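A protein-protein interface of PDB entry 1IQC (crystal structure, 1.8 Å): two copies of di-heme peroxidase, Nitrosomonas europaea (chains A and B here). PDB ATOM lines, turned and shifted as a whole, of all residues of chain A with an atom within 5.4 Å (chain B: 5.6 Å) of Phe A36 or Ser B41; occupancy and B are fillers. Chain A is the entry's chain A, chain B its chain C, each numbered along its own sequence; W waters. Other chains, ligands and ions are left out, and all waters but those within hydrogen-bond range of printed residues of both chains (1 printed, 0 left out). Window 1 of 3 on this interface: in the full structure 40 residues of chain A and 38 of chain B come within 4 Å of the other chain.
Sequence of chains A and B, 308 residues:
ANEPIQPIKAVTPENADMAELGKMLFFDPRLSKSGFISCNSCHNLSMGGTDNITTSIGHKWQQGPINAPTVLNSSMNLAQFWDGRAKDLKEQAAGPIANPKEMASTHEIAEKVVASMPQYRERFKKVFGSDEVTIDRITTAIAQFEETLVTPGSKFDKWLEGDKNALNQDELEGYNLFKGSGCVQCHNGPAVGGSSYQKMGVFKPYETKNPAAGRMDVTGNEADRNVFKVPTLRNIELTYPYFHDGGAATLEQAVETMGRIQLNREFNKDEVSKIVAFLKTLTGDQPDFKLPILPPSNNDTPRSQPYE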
ATOM      1  N   PRO A  29      27.034 -25.841  -4.950  1.00  0.00           N
ATOM      2  CA  PRO A  29      26.771 -26.799  -6.025  1.00  0.00           C
ATOM      3  C   PRO A  29      27.774 -26.743  -7.167  1.00  0.00           C
ATOM      4  O   PRO A  29      27.718 -27.572  -8.071  1.00  0.00           O
ATOM      5  CB  PRO A  29      25.364 -26.430  -6.476  1.00  0.00           C
ATOM      6  CG  PRO A  29      25.369 -24.946  -6.331  1.00  0.00           C
ATOM      7  CD  PRO A  29      26.045 -24.744  -4.974  1.00  0.00           C
ATOM      8  N   SER A  32      30.117 -29.595  -8.221  1.00  0.00           N
ATOM      9  CA  SER A  32      29.616 -30.612  -9.150  1.00  0.00           C
ATOM     10  C   SER A  32      29.736 -30.147 -10.598  1.00  0.00           C
ATOM     11  O   SER A  32      29.802 -28.950 -10.876  1.00  0.00           O
ATOM     12  CB  SER A  32      28.149 -30.948  -8.855  1.00  0.00           C
ATOM     13  OG  SER A  32      27.279 -29.908  -9.282  1.00  0.00           O
ATOM     14  N   SER A  34      27.479 -30.318 -12.954  1.00  0.00           N
ATOM     15  CA  SER A  34      26.243 -29.665 -13.360  1.00  0.00           C
ATOM     16  C   SER A  34      26.070 -28.288 -12.743  1.00  0.00           C
ATOM     17  O   SER A  34      25.327 -27.465 -13.271  1.00  0.00           O
ATOM     18  CB  SER A  34      25.049 -30.515 -12.942  1.00  0.00           C
ATOM     19  OG  SER A  34      24.998 -30.605 -11.525  1.00  0.00           O
ATOM     20  N   GLY A  35      26.743 -28.061 -11.620  1.00  0.00           N
ATOM     21  CA  GLY A  35      26.608 -26.803 -10.903  1.00  0.00           C
ATOM     22  C   GLY A  35      25.273 -26.817 -10.165  1.00  0.00           C
ATOM     23  O   GLY A  35      24.808 -25.781  -9.673  1.00  0.00           O
ATOM     24  N   PHE A  36      24.664 -27.997 -10.066  1.00  0.00           N
ATOM     25  CA  PHE A  36      23.341 -28.146  -9.432  1.00  0.00           C
ATOM     26  C   PHE A  36      23.315 -29.015  -8.181  1.00  0.00           C
ATOM     27  O   PHE A  36      22.360 -28.977  -7.404  1.00  0.00           O
ATOM     28  CB  PHE A  36      22.362 -28.726 -10.469  1.00  0.00           C
ATOM     29  CG  PHE A  36      20.923 -28.814 -10.006  1.00  0.00           C
ATOM     30  CD1 PHE A  36      20.210 -27.670  -9.668  1.00  0.00           C
ATOM     31  CD2 PHE A  36      20.261 -30.040  -9.980  1.00  0.00           C
ATOM     32  CE1 PHE A  36      18.853 -27.741  -9.316  1.00  0.00           C
ATOM     33  CE2 PHE A  36      18.913 -30.126  -9.631  1.00  0.00           C
ATOM     34  CZ  PHE A  36      18.203 -28.967  -9.298  1.00  0.00           C
ATOM     35  N   ILE A  37      24.365 -29.801  -7.991  1.00  0.00           N
ATOM     36  CA  ILE A  37      24.454 -30.714  -6.862  1.00  0.00           C
ATOM     37  C   ILE A  37      25.539 -30.331  -5.859  1.00  0.00           C
ATOM     38  O   ILE A  37      26.709 -30.170  -6.233  1.00  0.00           O
ATOM     39  CB  ILE A  37      24.749 -32.152  -7.373  1.00  0.00           C
ATOM     40  CG1 ILE A  37      23.606 -32.637  -8.267  1.00  0.00           C
ATOM     41  CG2 ILE A  37      24.979 -33.097  -6.201  1.00  0.00           C
ATOM     42  CD1 ILE A  37      23.877 -33.999  -8.919  1.00  0.00           C
ATOM     43  N   SER A  38      25.151 -30.173  -4.590  1.00  0.00           N
ATOM     44  CA  SER A  38      26.106 -29.873  -3.511  1.00  0.00           C
ATOM     45  C   SER A  38      26.061 -31.048  -2.521  1.00  0.00           C
ATOM     46  O   SER A  38      25.250 -31.963  -2.675  1.00  0.00           O
ATOM     47  CB  SER A  38      25.713 -28.590  -2.764  1.00  0.00           C
ATOM     48  OG  SER A  38      24.546 -28.799  -1.970  1.00  0.00           O
ATOM     49  N   SER A  41      22.736 -31.477  -1.149  1.00  0.00           N
ATOM     50  CA  SER A  41      21.687 -32.059  -1.983  1.00  0.00           C
ATOM     51  C   SER A  41      21.352 -33.475  -1.511  1.00  0.00           C
ATOM     52  O   SER A  41      20.183 -33.861  -1.447  1.00  0.00           O
ATOM     53  CB  SER A  41      22.135 -32.114  -3.445  1.00  0.00           C
ATOM     54  OG  SER A  41      22.383 -30.823  -3.957  1.00  0.00           O
ATOM     55  N   PHE B  36      13.150 -34.387  -3.939  1.00  0.00           N
ATOM     56  CA  PHE B  36      14.511 -33.879  -4.145  1.00  0.00           C
ATOM     57  C   PHE B  36      14.576 -32.413  -4.569  1.00  0.00           C
ATOM     58  O   PHE B  36      15.616 -31.775  -4.436  1.00  0.00           O
ATOM     59  CB  PHE B  36      15.190 -34.733  -5.225  1.00  0.00           C
ATOM     60  CG  PHE B  36      16.652 -34.427  -5.439  1.00  0.00           C
ATOM     61  CD1 PHE B  36      17.569 -34.577  -4.401  1.00  0.00           C
ATOM     62  CD2 PHE B  36      17.121 -34.066  -6.703  1.00  0.00           C
ATOM     63  CE1 PHE B  36      18.928 -34.383  -4.618  1.00  0.00           C
ATOM     64  CE2 PHE B  36      18.490 -33.868  -6.932  1.00  0.00           C
ATOM     65  CZ  PHE B  36      19.392 -34.031  -5.884  1.00  0.00           C
ATOM     66  N   ILE B  37      13.470 -31.889  -5.087  1.00  0.00           N
ATOM     67  CA  ILE B  37      13.435 -30.514  -5.579  1.00  0.00           C
ATOM     68  C   ILE B  37      12.571 -29.567  -4.739  1.00  0.00           C
ATOM     69  O   ILE B  37      11.400 -29.840  -4.493  1.00  0.00           O
ATOM     70  CB  ILE B  37      12.929 -30.499  -7.046  1.00  0.00           C
ATOM     71  CG1 ILE B  37      13.850 -31.368  -7.915  1.00  0.00           C
ATOM     72  CG2 ILE B  37      12.880 -29.080  -7.594  1.00  0.00           C
ATOM     73  CD1 ILE B  37      13.432 -31.428  -9.384  1.00  0.00           C
ATOM     74  N   SER B  38      13.167 -28.464  -4.293  1.00  0.00           N
ATOM     75  CA  SER B  38      12.452 -27.445  -3.510  1.00  0.00           C
ATOM     76  C   SER B  38      12.539 -26.140  -4.300  1.00  0.00           C
ATOM     77  O   SER B  38      13.190 -26.093  -5.345  1.00  0.00           O
ATOM     78  CB  SER B  38      13.120 -27.246  -2.144  1.00  0.00           C
ATOM     79  OG  SER B  38      14.390 -26.609  -2.282  1.00  0.00           O
ATOM     80  N   CYS B  39      11.898 -25.072  -3.819  1.00  0.00           N
ATOM     81  CA  CYS B  39      11.986 -23.799  -4.522  1.00  0.00           C
ATOM     82  C   CYS B  39      13.457 -23.367  -4.549  1.00  0.00           C
ATOM     83  O   CYS B  39      13.917 -22.759  -5.518  1.00  0.00           O
ATOM     84  CB  CYS B  39      11.209 -22.702  -3.792  1.00  0.00           C
ATOM     85  SG  CYS B  39       9.479 -23.054  -3.514  1.00  0.00           S
ATOM     86  N   ASN B  40      14.168 -23.672  -3.466  1.00  0.00           N
ATOM     87  CA  ASN B  40      15.565 -23.284  -3.315  1.00  0.00           C
ATOM     88  C   ASN B  40      16.477 -23.978  -4.318  1.00  0.00           C
ATOM     89  O   ASN B  40      17.541 -23.472  -4.622  1.00  0.00           O
ATOM     90  CB  ASN B  40      16.053 -23.575  -1.887  1.00  0.00           C
ATOM     91  CG  ASN B  40      17.386 -22.912  -1.574  1.00  0.00           C
ATOM     92  OD1 ASN B  40      18.407 -23.586  -1.401  1.00  0.00           O
ATOM     93  ND2 ASN B  40      17.384 -21.592  -1.497  1.00  0.00           N
ATOM     94  N   SER B  41      16.062 -25.135  -4.825  1.00  0.00           N
ATOM     95  CA  SER B  41      16.877 -25.846  -5.815  1.00  0.00           C
ATOM     96  C   SER B  41      17.090 -24.987  -7.055  1.00  0.00           C
ATOM     97  O   SER B  41      18.198 -24.919  -7.592  1.00  0.00           O
ATOM     98  CB  SER B  41      16.200 -27.156  -6.220  1.00  0.00           C
ATOM     99  OG  SER B  41      15.963 -27.966  -5.090  1.00  0.00           O
ATOM    100  N   CYS B  42      16.032 -24.329  -7.512  1.00  0.00           N
ATOM    101  CA  CYS B  42      16.114 -23.488  -8.703  1.00  0.00           C
ATOM    102  C   CYS B  42      16.291 -22.004  -8.429  1.00  0.00           C
ATOM    103  O   CYS B  42      16.641 -21.250  -9.327  1.00  0.00           O
ATOM    104  CB  CYS B  42      14.880 -23.689  -9.560  1.00  0.00           C
ATOM    105  SG  CYS B  42      14.766 -25.371 -10.226  1.00  0.00           S
ATOM    106  N   HIS B  43      16.045 -21.599  -7.189  1.00  0.00           N
ATOM    107  CA  HIS B  43      16.176 -20.199  -6.780  1.00  0.00           C
ATOM    108  C   HIS B  43      17.013 -20.265  -5.519  1.00  0.00           C
ATOM    109  O   HIS B  43      16.527 -20.040  -4.409  1.00  0.00           O
ATOM    110  CB  HIS B  43      14.794 -19.618  -6.478  1.00  0.00           C
ATOM    111  CG  HIS B  43      13.874 -19.619  -7.660  1.00  0.00           C
ATOM    112  ND1 HIS B  43      14.062 -18.795  -8.747  1.00  0.00           N
ATOM    113  CD2 HIS B  43      12.772 -20.357  -7.934  1.00  0.00           C
ATOM    114  CE1 HIS B  43      13.116 -19.024  -9.642  1.00  0.00           C
ATOM    115  NE2 HIS B  43      12.321 -19.968  -9.173  1.00  0.00           N
ATOM    116  N   ASN B  44      18.287 -20.584  -5.710  1.00  0.00           N
ATOM    117  CA  ASN B  44      19.215 -20.791  -4.606  1.00  0.00           C
ATOM    118  C   ASN B  44      19.568 -19.528  -3.833  1.00  0.00           C
ATOM    119  O   ASN B  44      20.329 -18.696  -4.305  1.00  0.00           O
ATOM    120  CB  ASN B  44      20.484 -21.461  -5.140  1.00  0.00           C
ATOM    121  CG  ASN B  44      21.304 -22.092  -4.043  1.00  0.00           C
ATOM    122  OD1 ASN B  44      21.475 -21.506  -2.979  1.00  0.00           O
ATOM    123  ND2 ASN B  44      21.822 -23.296  -4.295  1.00  0.00           N
ATOM    124  N   THR B  50      18.791 -17.831  -7.971  1.00  0.00           N
ATOM    125  CA  THR B  50      18.549 -18.515  -9.253  1.00  0.00           C
ATOM    126  C   THR B  50      19.336 -19.822  -9.242  1.00  0.00           C
ATOM    127  O   THR B  50      19.893 -20.189  -8.212  1.00  0.00           O
ATOM    128  CB  THR B  50      19.007 -17.677 -10.475  1.00  0.00           C
ATOM    129  OG1 THR B  50      20.436 -17.756 -10.622  1.00  0.00           O
ATOM    130  CG2 THR B  50      18.607 -16.217 -10.314  1.00  0.00           C
ATOM    131  N   ASP B  51      19.375 -20.534 -10.366  1.00  0.00           N
ATOM    132  CA  ASP B  51      20.131 -21.784 -10.410  1.00  0.00           C
ATOM    133  C   ASP B  51      21.422 -21.654 -11.212  1.00  0.00           C
ATOM    134  O   ASP B  51      22.163 -22.624 -11.385  1.00  0.00           O
ATOM    135  CB  ASP B  51      19.280 -22.935 -10.958  1.00  0.00           C
ATOM    136  CG  ASP B  51      18.616 -22.608 -12.274  1.00  0.00           C
ATOM    137  OD1 ASP B  51      19.108 -21.726 -13.005  1.00  0.00           O
ATOM    138  OD2 ASP B  51      17.602 -23.267 -12.580  1.00  0.00           O
ATOM    139  N   ILE B  53      22.290 -21.540 -14.307  1.00  0.00           N
ATOM    140  CA  ILE B  53      22.520 -22.384 -15.478  1.00  0.00           C
ATOM    141  C   ILE B  53      21.586 -21.878 -16.581  1.00  0.00           C
ATOM    142  O   ILE B  53      20.665 -21.106 -16.301  1.00  0.00           O
ATOM    143  CB  ILE B  53      22.299 -23.886 -15.179  1.00  0.00           C
ATOM    144  CG1 ILE B  53      20.930 -24.128 -14.542  1.00  0.00           C
ATOM    145  CG2 ILE B  53      23.420 -24.387 -14.286  1.00  0.00           C
ATOM    146  CD1 ILE B  53      20.605 -25.611 -14.339  1.00  0.00           C
ATOM    147  N   ILE B  57      16.845 -27.372 -14.346  1.00  0.00           N
ATOM    148  CA  ILE B  57      16.829 -28.832 -14.291  1.00  0.00           C
ATOM    149  C   ILE B  57      15.578 -29.196 -13.483  1.00  0.00           C
ATOM    150  O   ILE B  57      15.458 -28.806 -12.318  1.00  0.00           O
ATOM    151  CB  ILE B  57      18.071 -29.367 -13.526  1.00  0.00           C
ATOM    152  CG1 ILE B  57      19.339 -29.107 -14.339  1.00  0.00           C
ATOM    153  CG2 ILE B  57      17.900 -30.850 -13.216  1.00  0.00           C
ATOM    154  CD1 ILE B  57      20.620 -29.379 -13.567  1.00  0.00           C
ATOM    155  N   TRP B  61      15.629 -34.738 -14.361  1.00  0.00           N
ATOM    156  CA  TRP B  61      16.605 -33.964 -15.123  1.00  0.00           C
ATOM    157  C   TRP B  61      16.102 -33.430 -16.457  1.00  0.00           C
ATOM    158  O   TRP B  61      16.838 -33.384 -17.444  1.00  0.00           O
ATOM    159  CB  TRP B  61      17.891 -34.784 -15.326  1.00  0.00           C
ATOM    160  CG  TRP B  61      19.165 -33.957 -15.349  1.00  0.00           C
ATOM    161  CD1 TRP B  61      19.745 -33.360 -16.434  1.00  0.00           C
ATOM    162  CD2 TRP B  61      20.027 -33.679 -14.235  1.00  0.00           C
ATOM    163  NE1 TRP B  61      20.913 -32.738 -16.069  1.00  0.00           N
ATOM    164  CE2 TRP B  61      21.111 -32.918 -14.724  1.00  0.00           C
ATOM    165  CE3 TRP B  61      19.989 -34.005 -12.873  1.00  0.00           C
ATOM    166  CZ2 TRP B  61      22.153 -32.478 -13.896  1.00  0.00           C
ATOM    167  CZ3 TRP B  61      21.027 -33.567 -12.050  1.00  0.00           C
ATOM    168  CH2 TRP B  61      22.092 -32.813 -12.566  1.00  0.00           C
HETATM  169  O   HOH W   1      22.317 -24.513  -9.345  1.00  0.00           O
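N of Ser B38 is in hydrogen-bond range of OG of Ser B41, at 2.9 Å.
OG of Ser A32 lies within hydrogen-bond range of OG of Ser A34 (3.3 Å).
The side-chain hydroxyl (OG) of Ser A32 sits at hydrogen-bond distance from the backbone NH (N) of Phe A36, 3.3 Å away.
The side-chain hydroxyl (OG) of Ser A34 lies within hydrogen-bond range of the backbone NH (N) of Phe A36 (3.0 Å).
N of Ser A38 is in hydrogen-bond range of OG of Ser A41, at 2.9 Å.
OD1 of Asp B51 lies close to N of Ile B53 (3.4 Å).
Phe A36 touches Ser B41, and with the chains exchanged Ser A41 touches Phe B36.
Of the 5 pairs that touch across the chains among the printed residues, 2 have their exchanged pair printed and touching as well.
Of the 14 printed residues of chain B, 5 touch a printed residue of chain A.
Hydrophobic or aromatic side chains of chain B that line the printed part of chain A: Phe B36, Ile B53, Ile B57 and Trp B61.
Printed residues of chain A that touch a printed residue of chain B: Ser A34, Phe A36 and Ser A41.
Hydrophobic or aromatic side chains of chain A within 4 Å of the printed part of chain B: Phe A36.
Water W1 lies within hydrogen-bond range of the backbone carbonyl oxygen (O) of Asp B51 and the backbone carbonyl oxygen (O) of Gly A35.
Among the printed residues, pairs that only touch across the chains: Phe A36 with Ser B41, Ser A41 with Phe B36, Phe A36 with Ile B57, Ser A34 with Trp B61 and Ser A34 with Ile B53.
Of chain B, only Ser B41 and Ile B57 come within 4 Å of Phe A36.
Of chain A, only Phe A36 (3.4 Å) comes within 4 Å of Ser B41.
Of the printed residues of chain A, Ile B57 touches Phe A36.
Printed residues of chain B within 4 Å of Ser A41: Phe B36 (3.5 Å).
Of the printed residues of chain A, Ile B53 touches Ser A34.
Printed residues of chain B within 4 Å of Ser A34: Ile B53 and Trp B61.
Of the printed residues of chain A, Phe B36 touches Ser A41 (3.5 Å).
Thr B50 touches none of the printed residues of chain A.
The nearest printed residue of chain A that does not touch Ser B41 is Gly A35 (7.0 Å).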
